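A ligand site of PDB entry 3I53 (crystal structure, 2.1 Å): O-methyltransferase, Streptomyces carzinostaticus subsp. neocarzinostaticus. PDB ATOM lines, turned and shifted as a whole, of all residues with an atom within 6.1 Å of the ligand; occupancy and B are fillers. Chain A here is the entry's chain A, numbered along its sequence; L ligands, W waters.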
ATOM      1  N   TRP A 133     -23.438 -26.795 -33.036  1.00  0.00           N
ATOM      2  CA  TRP A 133     -22.453 -25.966 -32.341  1.00  0.00           C
ATOM      3  C   TRP A 133     -21.978 -24.781 -33.203  1.00  0.00           C
ATOM      4  O   TRP A 133     -21.827 -23.669 -32.700  1.00  0.00           O
ATOM      5  CB  TRP A 133     -21.241 -26.813 -31.917  1.00  0.00           C
ATOM      6  CG  TRP A 133     -21.585 -27.874 -30.923  1.00  0.00           C
ATOM      7  CD1 TRP A 133     -21.306 -29.216 -31.023  1.00  0.00           C
ATOM      8  CD2 TRP A 133     -22.352 -27.709 -29.723  1.00  0.00           C
ATOM      9  NE1 TRP A 133     -21.857 -29.888 -29.969  1.00  0.00           N
ATOM     10  CE2 TRP A 133     -22.506 -28.997 -29.154  1.00  0.00           C
ATOM     11  CE3 TRP A 133     -22.923 -26.605 -29.084  1.00  0.00           C
ATOM     12  CZ2 TRP A 133     -23.213 -29.204 -27.976  1.00  0.00           C
ATOM     13  CZ3 TRP A 133     -23.632 -26.822 -27.903  1.00  0.00           C
ATOM     14  CH2 TRP A 133     -23.768 -28.110 -27.361  1.00  0.00           C
ATOM     15  N   PHE A 146     -29.725 -21.586 -25.848  1.00  0.00           N
ATOM     16  CA  PHE A 146     -29.301 -22.899 -25.405  1.00  0.00           C
ATOM     17  C   PHE A 146     -28.826 -22.832 -23.943  1.00  0.00           C
ATOM     18  O   PHE A 146     -29.145 -23.716 -23.157  1.00  0.00           O
ATOM     19  CB  PHE A 146     -28.173 -23.437 -26.299  1.00  0.00           C
ATOM     20  CG  PHE A 146     -27.738 -24.837 -25.939  1.00  0.00           C
ATOM     21  CD1 PHE A 146     -28.503 -25.937 -26.321  1.00  0.00           C
ATOM     22  CD2 PHE A 146     -26.575 -25.055 -25.203  1.00  0.00           C
ATOM     23  CE1 PHE A 146     -28.120 -27.238 -25.959  1.00  0.00           C
ATOM     24  CE2 PHE A 146     -26.178 -26.338 -24.840  1.00  0.00           C
ATOM     25  CZ  PHE A 146     -26.956 -27.434 -25.220  1.00  0.00           C
ATOM     26  N   MET A 150     -30.202 -24.901 -20.784  1.00  0.00           N
ATOM     27  CA  MET A 150     -29.366 -25.751 -19.946  1.00  0.00           C
ATOM     28  C   MET A 150     -29.543 -25.391 -18.478  1.00  0.00           C
ATOM     29  O   MET A 150     -29.645 -26.272 -17.618  1.00  0.00           O
ATOM     30  CB  MET A 150     -27.885 -25.621 -20.328  1.00  0.00           C
ATOM     31  CG  MET A 150     -27.514 -26.294 -21.646  1.00  0.00           C
ATOM     32  SD  MET A 150     -27.817 -28.085 -21.653  1.00  0.00           S
ATOM     33  CE  MET A 150     -29.382 -28.158 -22.449  1.00  0.00           C
ATOM     34  N   SER A 151     -29.586 -24.107 -18.181  1.00  0.00           N
ATOM     35  CA  SER A 151     -29.776 -23.660 -16.806  1.00  0.00           C
ATOM     36  C   SER A 151     -31.017 -24.324 -16.216  1.00  0.00           C
ATOM     37  O   SER A 151     -31.070 -24.652 -15.039  1.00  0.00           O
ATOM     38  CB  SER A 151     -29.919 -22.143 -16.755  1.00  0.00           C
ATOM     39  OG  SER A 151     -30.070 -21.695 -15.420  1.00  0.00           O
ATOM     40  N   HIS A 153     -32.146 -27.207 -17.124  1.00  0.00           N
ATOM     41  CA  HIS A 153     -31.793 -28.597 -16.945  1.00  0.00           C
ATOM     42  C   HIS A 153     -31.005 -28.759 -15.643  1.00  0.00           C
ATOM     43  O   HIS A 153     -31.187 -29.724 -14.911  1.00  0.00           O
ATOM     44  CB  HIS A 153     -30.975 -29.106 -18.147  1.00  0.00           C
ATOM     45  CG  HIS A 153     -29.595 -29.590 -17.791  1.00  0.00           C
ATOM     46  ND1 HIS A 153     -28.507 -28.745 -17.713  1.00  0.00           N
ATOM     47  CD2 HIS A 153     -29.128 -30.830 -17.526  1.00  0.00           C
ATOM     48  CE1 HIS A 153     -27.430 -29.448 -17.409  1.00  0.00           C
ATOM     49  NE2 HIS A 153     -27.779 -30.717 -17.284  1.00  0.00           N
ATOM     50  N   LEU A 154     -30.129 -27.797 -15.358  1.00  0.00           N
ATOM     51  CA  LEU A 154     -29.329 -27.823 -14.142  1.00  0.00           C
ATOM     52  C   LEU A 154     -30.209 -27.777 -12.901  1.00  0.00           C
ATOM     53  O   LEU A 154     -29.962 -28.478 -11.920  1.00  0.00           O
ATOM     54  CB  LEU A 154     -28.345 -26.647 -14.128  1.00  0.00           C
ATOM     55  CG  LEU A 154     -27.152 -26.712 -15.101  1.00  0.00           C
ATOM     56  CD1 LEU A 154     -26.404 -25.378 -15.088  1.00  0.00           C
ATOM     57  CD2 LEU A 154     -26.219 -27.848 -14.684  1.00  0.00           C
ATOM     58  N   TYR A 158     -29.855 -31.025 -10.821  1.00  0.00           N
ATOM     59  CA  TYR A 158     -28.636 -30.726 -10.086  1.00  0.00           C
ATOM     60  C   TYR A 158     -28.772 -30.074  -8.725  1.00  0.00           C
ATOM     61  O   TYR A 158     -27.779 -29.874  -8.030  1.00  0.00           O
ATOM     62  CB  TYR A 158     -27.683 -29.884 -10.957  1.00  0.00           C
ATOM     63  CG  TYR A 158     -27.060 -30.629 -12.123  1.00  0.00           C
ATOM     64  CD1 TYR A 158     -27.812 -31.486 -12.935  1.00  0.00           C
ATOM     65  CD2 TYR A 158     -25.716 -30.440 -12.453  1.00  0.00           C
ATOM     66  CE1 TYR A 158     -27.257 -32.123 -14.037  1.00  0.00           C
ATOM     67  CE2 TYR A 158     -25.148 -31.075 -13.574  1.00  0.00           C
ATOM     68  CZ  TYR A 158     -25.923 -31.906 -14.348  1.00  0.00           C
ATOM     69  OH  TYR A 158     -25.392 -32.519 -15.464  1.00  0.00           O
ATOM     70  N   ASP A 175     -14.353 -28.108 -15.198  1.00  0.00           N
ATOM     71  CA  ASP A 175     -15.607 -28.488 -15.821  1.00  0.00           C
ATOM     72  C   ASP A 175     -15.408 -28.431 -17.346  1.00  0.00           C
ATOM     73  O   ASP A 175     -15.449 -27.364 -17.947  1.00  0.00           O
ATOM     74  CB  ASP A 175     -16.730 -27.542 -15.391  1.00  0.00           C
ATOM     75  CG  ASP A 175     -18.105 -28.133 -15.616  1.00  0.00           C
ATOM     76  OD1 ASP A 175     -18.212 -29.059 -16.443  1.00  0.00           O
ATOM     77  OD2 ASP A 175     -19.096 -27.675 -14.990  1.00  0.00           O
ATOM     78  N   VAL A 176     -15.197 -29.600 -17.948  1.00  0.00           N
ATOM     79  CA  VAL A 176     -14.955 -29.753 -19.372  1.00  0.00           C
ATOM     80  C   VAL A 176     -16.265 -29.659 -20.162  1.00  0.00           C
ATOM     81  O   VAL A 176     -17.096 -30.573 -20.112  1.00  0.00           O
ATOM     82  CB  VAL A 176     -14.269 -31.108 -19.647  1.00  0.00           C
ATOM     83  CG1 VAL A 176     -13.815 -31.195 -21.090  1.00  0.00           C
ATOM     84  CG2 VAL A 176     -13.100 -31.286 -18.698  1.00  0.00           C
ATOM     85  N   GLY A 177     -16.411 -28.578 -20.910  1.00  0.00           N
ATOM     86  CA  GLY A 177     -17.644 -28.342 -21.648  1.00  0.00           C
ATOM     87  C   GLY A 177     -18.597 -27.814 -20.601  1.00  0.00           C
ATOM     88  O   GLY A 177     -19.781 -28.107 -20.614  1.00  0.00           O
ATOM     89  N   GLY A 178     -18.065 -27.001 -19.685  1.00  0.00           N
ATOM     90  CA  GLY A 178     -18.864 -26.461 -18.596  1.00  0.00           C
ATOM     91  C   GLY A 178     -19.897 -25.377 -18.853  1.00  0.00           C
ATOM     92  O   GLY A 178     -20.469 -24.846 -17.905  1.00  0.00           O
ATOM     93  N   GLY A 179     -20.139 -25.031 -20.111  1.00  0.00           N
ATOM     94  CA  GLY A 179     -21.137 -24.015 -20.395  1.00  0.00           C
ATOM     95  C   GLY A 179     -20.865 -22.653 -19.780  1.00  0.00           C
ATOM     96  O   GLY A 179     -19.711 -22.191 -19.716  1.00  0.00           O
ATOM     97  N   SER A 180     -21.924 -21.996 -19.329  1.00  0.00           N
ATOM     98  CA  SER A 180     -21.816 -20.668 -18.728  1.00  0.00           C
ATOM     99  C   SER A 180     -21.399 -20.736 -17.273  1.00  0.00           C
ATOM    100  O   SER A 180     -21.470 -19.745 -16.548  1.00  0.00           O
ATOM    101  CB  SER A 180     -23.153 -19.939 -18.858  1.00  0.00           C
ATOM    102  OG  SER A 180     -24.171 -20.617 -18.171  1.00  0.00           O
ATOM    103  N   LEU A 183     -22.932 -24.914 -13.074  1.00  0.00           N
ATOM    104  CA  LEU A 183     -22.549 -25.984 -12.156  1.00  0.00           C
ATOM    105  C   LEU A 183     -21.357 -25.613 -11.280  1.00  0.00           C
ATOM    106  O   LEU A 183     -21.372 -25.815 -10.068  1.00  0.00           O
ATOM    107  CB  LEU A 183     -22.218 -27.277 -12.918  1.00  0.00           C
ATOM    108  CG  LEU A 183     -21.578 -28.394 -12.082  1.00  0.00           C
ATOM    109  CD1 LEU A 183     -22.532 -28.826 -10.967  1.00  0.00           C
ATOM    110  CD2 LEU A 183     -21.219 -29.566 -12.976  1.00  0.00           C
ATOM    111  N   LEU A 199     -14.000 -24.809 -18.968  1.00  0.00           N
ATOM    112  CA  LEU A 199     -13.349 -24.955 -20.262  1.00  0.00           C
ATOM    113  C   LEU A 199     -14.467 -25.134 -21.270  1.00  0.00           C
ATOM    114  O   LEU A 199     -15.243 -26.086 -21.182  1.00  0.00           O
ATOM    115  CB  LEU A 199     -12.409 -26.163 -20.263  1.00  0.00           C
ATOM    116  CG  LEU A 199     -11.608 -26.493 -21.537  1.00  0.00           C
ATOM    117  CD1 LEU A 199     -12.540 -27.017 -22.624  1.00  0.00           C
ATOM    118  CD2 LEU A 199     -10.849 -25.284 -22.029  1.00  0.00           C
ATOM    119  N   ASP A 200     -14.588 -24.201 -22.204  1.00  0.00           N
ATOM    120  CA  ASP A 200     -15.611 -24.282 -23.230  1.00  0.00           C
ATOM    121  C   ASP A 200     -15.266 -23.374 -24.411  1.00  0.00           C
ATOM    122  O   ASP A 200     -14.150 -22.852 -24.496  1.00  0.00           O
ATOM    123  CB  ASP A 200     -16.976 -23.885 -22.653  1.00  0.00           C
ATOM    124  CG  ASP A 200     -18.146 -24.566 -23.375  1.00  0.00           C
ATOM    125  OD1 ASP A 200     -18.368 -24.272 -24.562  1.00  0.00           O
ATOM    126  OD2 ASP A 200     -18.822 -25.415 -22.753  1.00  0.00           O
ATOM    127  N   LEU A 201     -16.209 -23.193 -25.318  1.00  0.00           N
ATOM    128  CA  LEU A 201     -15.978 -22.346 -26.483  1.00  0.00           C
ATOM    129  C   LEU A 201     -16.175 -20.898 -26.075  1.00  0.00           C
ATOM    130  O   LEU A 201     -16.705 -20.623 -24.995  1.00  0.00           O
ATOM    131  CB  LEU A 201     -16.957 -22.738 -27.604  1.00  0.00           C
ATOM    132  CG  LEU A 201     -16.955 -24.254 -27.895  1.00  0.00           C
ATOM    133  CD1 LEU A 201     -18.102 -24.611 -28.835  1.00  0.00           C
ATOM    134  CD2 LEU A 201     -15.610 -24.659 -28.482  1.00  0.00           C
ATOM    135  N   PRO A 204     -19.947 -19.751 -24.395  1.00  0.00           N
ATOM    136  CA  PRO A 204     -20.232 -20.104 -23.003  1.00  0.00           C
ATOM    137  C   PRO A 204     -19.160 -19.593 -22.036  1.00  0.00           C
ATOM    138  O   PRO A 204     -19.479 -19.061 -20.978  1.00  0.00           O
ATOM    139  CB  PRO A 204     -20.295 -21.631 -23.056  1.00  0.00           C
ATOM    140  CG  PRO A 204     -20.850 -21.888 -24.427  1.00  0.00           C
ATOM    141  CD  PRO A 204     -19.995 -20.947 -25.262  1.00  0.00           C
ATOM    142  N   GLY A 226     -11.184 -23.037 -25.064  1.00  0.00           N
ATOM    143  CA  GLY A 226     -10.433 -24.078 -25.728  1.00  0.00           C
ATOM    144  C   GLY A 226     -11.335 -25.220 -26.129  1.00  0.00           C
ATOM    145  O   GLY A 226     -12.494 -25.277 -25.711  1.00  0.00           O
ATOM    146  N   SER A 227     -10.825 -26.118 -26.953  1.00  0.00           N
ATOM    147  CA  SER A 227     -11.610 -27.249 -27.399  1.00  0.00           C
ATOM    148  C   SER A 227     -11.266 -28.476 -26.553  1.00  0.00           C
ATOM    149  O   SER A 227     -10.086 -28.734 -26.316  1.00  0.00           O
ATOM    150  CB  SER A 227     -11.313 -27.542 -28.855  1.00  0.00           C
ATOM    151  OG  SER A 227     -11.951 -28.741 -29.242  1.00  0.00           O
ATOM    152  N   PHE A 228     -12.280 -29.222 -26.099  1.00  0.00           N
ATOM    153  CA  PHE A 228     -11.954 -30.389 -25.289  1.00  0.00           C
ATOM    154  C   PHE A 228     -11.390 -31.562 -26.092  1.00  0.00           C
ATOM    155  O   PHE A 228     -11.222 -32.653 -25.539  1.00  0.00           O
ATOM    156  CB  PHE A 228     -13.130 -30.835 -24.385  1.00  0.00           C
ATOM    157  CG  PHE A 228     -14.490 -30.855 -25.047  1.00  0.00           C
ATOM    158  CD1 PHE A 228     -14.690 -31.415 -26.308  1.00  0.00           C
ATOM    159  CD2 PHE A 228     -15.609 -30.367 -24.352  1.00  0.00           C
ATOM    160  CE1 PHE A 228     -15.978 -31.483 -26.868  1.00  0.00           C
ATOM    161  CE2 PHE A 228     -16.892 -30.446 -24.904  1.00  0.00           C
ATOM    162  CZ  PHE A 228     -17.081 -30.996 -26.162  1.00  0.00           C
ATOM    163  N   PHE A 229     -11.084 -31.348 -27.376  1.00  0.00           N
ATOM    164  CA  PHE A 229     -10.472 -32.418 -28.179  1.00  0.00           C
ATOM    165  C   PHE A 229      -8.954 -32.191 -28.115  1.00  0.00           C
ATOM    166  O   PHE A 229      -8.175 -33.056 -28.507  1.00  0.00           O
ATOM    167  CB  PHE A 229     -10.950 -32.399 -29.640  1.00  0.00           C
ATOM    168  CG  PHE A 229     -12.380 -32.835 -29.812  1.00  0.00           C
ATOM    169  CD1 PHE A 229     -13.381 -31.903 -30.051  1.00  0.00           C
ATOM    170  CD2 PHE A 229     -12.720 -34.171 -29.693  1.00  0.00           C
ATOM    171  CE1 PHE A 229     -14.712 -32.305 -30.150  1.00  0.00           C
ATOM    172  CE2 PHE A 229     -14.048 -34.586 -29.797  1.00  0.00           C
ATOM    173  CZ  PHE A 229     -15.044 -33.642 -30.024  1.00  0.00           C
ATOM    174  N   LEU A 241     -17.577 -33.873 -16.710  1.00  0.00           N
ATOM    175  CA  LEU A 241     -18.183 -33.935 -18.030  1.00  0.00           C
ATOM    176  C   LEU A 241     -19.679 -33.958 -17.752  1.00  0.00           C
ATOM    177  O   LEU A 241     -20.275 -35.017 -17.606  1.00  0.00           O
ATOM    178  CB  LEU A 241     -17.760 -35.207 -18.781  1.00  0.00           C
ATOM    179  CG  LEU A 241     -16.327 -35.211 -19.327  1.00  0.00           C
ATOM    180  CD1 LEU A 241     -15.942 -36.612 -19.774  1.00  0.00           C
ATOM    181  CD2 LEU A 241     -16.233 -34.208 -20.480  1.00  0.00           C
ATOM    182  N   SER A 242     -20.255 -32.763 -17.666  1.00  0.00           N
ATOM    183  CA  SER A 242     -21.685 -32.585 -17.365  1.00  0.00           C
ATOM    184  C   SER A 242     -22.530 -32.462 -18.625  1.00  0.00           C
ATOM    185  O   SER A 242     -22.483 -31.435 -19.291  1.00  0.00           O
ATOM    186  CB  SER A 242     -21.881 -31.326 -16.503  1.00  0.00           C
ATOM    187  OG  SER A 242     -23.250 -31.053 -16.315  1.00  0.00           O
ATOM    188  N   ALA A 243     -23.311 -33.494 -18.919  1.00  0.00           N
ATOM    189  CA  ALA A 243     -24.170 -33.487 -20.103  1.00  0.00           C
ATOM    190  C   ALA A 243     -23.383 -33.178 -21.385  1.00  0.00           C
ATOM    191  O   ALA A 243     -23.807 -32.377 -22.232  1.00  0.00           O
ATOM    192  CB  ALA A 243     -25.326 -32.498 -19.924  1.00  0.00           C
ATOM    193  N   VAL A 244     -22.220 -33.808 -21.520  1.00  0.00           N
ATOM    194  CA  VAL A 244     -21.363 -33.606 -22.688  1.00  0.00           C
ATOM    195  C   VAL A 244     -21.249 -34.849 -23.571  1.00  0.00           C
ATOM    196  O   VAL A 244     -21.574 -34.792 -24.751  1.00  0.00           O
ATOM    197  CB  VAL A 244     -19.931 -33.193 -22.254  1.00  0.00           C
ATOM    198  CG1 VAL A 244     -18.988 -33.225 -23.460  1.00  0.00           C
ATOM    199  CG2 VAL A 244     -19.945 -31.808 -21.642  1.00  0.00           C
ATOM    200  N   ASP A 247     -23.566 -36.001 -26.364  1.00  0.00           N
ATOM    201  CA  ASP A 247     -23.570 -35.112 -27.531  1.00  0.00           C
ATOM    202  C   ASP A 247     -22.654 -35.655 -28.633  1.00  0.00           C
ATOM    203  O   ASP A 247     -22.637 -35.142 -29.747  1.00  0.00           O
ATOM    204  CB  ASP A 247     -23.044 -33.723 -27.181  1.00  0.00           C
ATOM    205  CG  ASP A 247     -23.890 -33.005 -26.157  1.00  0.00           C
ATOM    206  OD1 ASP A 247     -23.458 -31.912 -25.731  1.00  0.00           O
ATOM    207  OD2 ASP A 247     -24.972 -33.518 -25.779  1.00  0.00           O
ATOM    208  N   TRP A 248     -21.895 -36.685 -28.320  1.00  0.00           N
ATOM    209  CA  TRP A 248     -20.951 -37.222 -29.282  1.00  0.00           C
ATOM    210  C   TRP A 248     -21.057 -38.713 -29.588  1.00  0.00           C
ATOM    211  O   TRP A 248     -21.618 -39.501 -28.806  1.00  0.00           O
ATOM    212  CB  TRP A 248     -19.530 -36.892 -28.808  1.00  0.00           C
ATOM    213  CG  TRP A 248     -19.334 -35.439 -28.516  1.00  0.00           C
ATOM    214  CD1 TRP A 248     -19.522 -34.804 -27.330  1.00  0.00           C
ATOM    215  CD2 TRP A 248     -18.947 -34.419 -29.454  1.00  0.00           C
ATOM    216  NE1 TRP A 248     -19.286 -33.463 -27.456  1.00  0.00           N
ATOM    217  CE2 TRP A 248     -18.930 -33.202 -28.753  1.00  0.00           C
ATOM    218  CE3 TRP A 248     -18.618 -34.422 -30.822  1.00  0.00           C
ATOM    219  CZ2 TRP A 248     -18.593 -31.974 -29.369  1.00  0.00           C
ATOM    220  CZ3 TRP A 248     -18.284 -33.204 -31.435  1.00  0.00           C
ATOM    221  CH2 TRP A 248     -18.268 -32.010 -30.701  1.00  0.00           C
HETATM  222  N1  LIG L   1     -21.731 -28.894 -18.632  1.00  0.00           N
HETATM  223  C1  LIG L   1     -22.723 -28.118 -19.376  1.00  0.00           C
HETATM  224  C2  LIG L   1     -22.874 -28.763 -20.759  1.00  0.00           C
HETATM  225  C3  LIG L   1     -23.675 -27.877 -21.715  1.00  0.00           C
HETATM  226  S1  LIG L   1     -24.066 -28.717 -23.295  1.00  0.00           S
HETATM  227  C4  LIG L   1     -24.064 -28.154 -18.630  1.00  0.00           C
HETATM  228  O1  LIG L   1     -24.240 -29.094 -17.831  1.00  0.00           O
HETATM  229  O2  LIG L   1     -24.888 -27.236 -18.864  1.00  0.00           O
HETATM  230  C5  LIG L   1     -22.428 -29.206 -23.950  1.00  0.00           C
HETATM  231  C6  LIG L   1     -21.331 -28.140 -23.870  1.00  0.00           C
HETATM  232  O3  LIG L   1     -20.218 -28.596 -24.658  1.00  0.00           O
HETATM  233  C7  LIG L   1     -21.772 -26.795 -24.462  1.00  0.00           C
HETATM  234  O4  LIG L   1     -21.451 -25.736 -23.554  1.00  0.00           O
HETATM  235  C8  LIG L   1     -20.929 -26.678 -25.730  1.00  0.00           C
HETATM  236  O5  LIG L   1     -20.593 -25.314 -25.965  1.00  0.00           O
HETATM  237  C9  LIG L   1     -19.674 -27.410 -25.264  1.00  0.00           C
HETATM  238  N2  LIG L   1     -18.785 -27.752 -26.402  1.00  0.00           N
HETATM  239  C10 LIG L   1     -19.155 -28.218 -27.596  1.00  0.00           C
HETATM  240  N3  LIG L   1     -18.070 -28.460 -28.326  1.00  0.00           N
HETATM  241  C11 LIG L   1     -17.002 -28.156 -27.602  1.00  0.00           C
HETATM  242  C12 LIG L   1     -15.632 -28.250 -27.800  1.00  0.00           C
HETATM  243  N4  LIG L   1     -15.137 -28.781 -28.922  1.00  0.00           N
HETATM  244  N5  LIG L   1     -14.805 -27.882 -26.815  1.00  0.00           N
HETATM  245  C13 LIG L   1     -15.268 -27.438 -25.663  1.00  0.00           C
HETATM  246  N6  LIG L   1     -16.573 -27.343 -25.436  1.00  0.00           N
HETATM  247  C14 LIG L   1     -17.455 -27.696 -26.374  1.00  0.00           C
HETATM  248  O   HOH W   1     -20.653 -31.090 -26.138  1.00  0.00           O
HETATM  249  O   HOH W   2     -17.725 -28.663 -31.205  1.00  0.00           O
HETATM  250  O   HOH W   3     -23.410 -23.959 -23.067  1.00  0.00           O
HETATM  251  O   HOH W   4     -21.865 -23.645 -27.627  1.00  0.00           O
HETATM  252  O   HOH W   5     -14.191 -27.632 -31.962  1.00  0.00           O
HETATM  253  O   HOH W   6     -21.362 -27.976 -16.272  1.00  0.00           O
HETATM  254  O   HOH W   7     -19.131 -30.347 -18.260  1.00  0.00           O
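N of Phe 228 is in hydrogen-bond range of N5 of the ligand (2.9 Å). OG of Ser 242 is in hydrogen-bond range of O1 of the ligand, at 2.7 Å. OG of Ser 227 is in hydrogen-bond range of N4 of the ligand. O of Gly 177 sits at hydrogen-bond distance from N1 of the ligand (2.9 Å). A nitrogen (N1) of the ligand lies within hydrogen-bond range of the backbone carbonyl oxygen of Ser 242 (2.7 Å). The side-chain carboxylate of Asp 200 is in hydrogen-bond range of an oxygen (O4) of the ligand, 2.8 Å away.
The backbone NH of Gly 179 lies within hydrogen-bond range of the side-chain carboxylate of Asp 200, 3.0 Å away. A ring nitrogen (ND1) of His 153 sits at hydrogen-bond distance from the backbone carbonyl oxygen (O) of Met 150 (2.7 Å). The backbone NH (N) of Gly 178 lies within hydrogen-bond range of the backbone carbonyl oxygen (O) of Leu 199 (3.3 Å). N of Phe 229 sits close to OG of Ser 227 (3.3 Å). The backbone carbonyl oxygen (O) of Asp 200 lies within hydrogen-bond range of the backbone NH (N) of Gly 226, at 3.0 Å. OH of Tyr 158 sits at hydrogen-bond distance from OG of Ser 242, 2.7 Å away. N of Gly 177 is in hydrogen-bond range of O of Leu 199 (2.8 Å).
Residues that only touch the ligand: Trp 133 (3.5 Å), Phe 146 (3.5 Å), Met 150 (3.7 Å), His 153 (3.2 Å), Leu 154 (3.9 Å), Gly 178 (3.8 Å), Gly 179 (3.6 Å), Leu 201 (3.7 Å), Pro 204 (3.8 Å), Gly 226 (3.5 Å), Phe 229 (3.8 Å), Ala 243 (3.8 Å), Asp 247 (3.4 Å) and Trp 248 (3.7 Å). Hydrophobic or aromatic side chains within 4 Å of the ligand: Trp 133, Phe 146, Met 150, His 153, Leu 154, Leu 201, Pro 204, Phe 228, Phe 229 and Trp 248. 19 residues have an atom within 4 Å of the ligand: Trp 133, Phe 146, Met 150, His 153, Leu 154, Gly 177, Gly 178, Gly 179, Asp 200, Leu 201, Pro 204, Gly 226, Ser 227, Phe 228, Phe 229, Ser 242, Ala 243, Asp 247 and Trp 248.
Water W6 bridges N1 of the ligand (2.6 Å) and OD2 of Asp 175 (2.6 Å). Water W1 lies within hydrogen-bond range of O3 of the ligand, OD1 of Asp 247 and NE1 of Trp 248.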
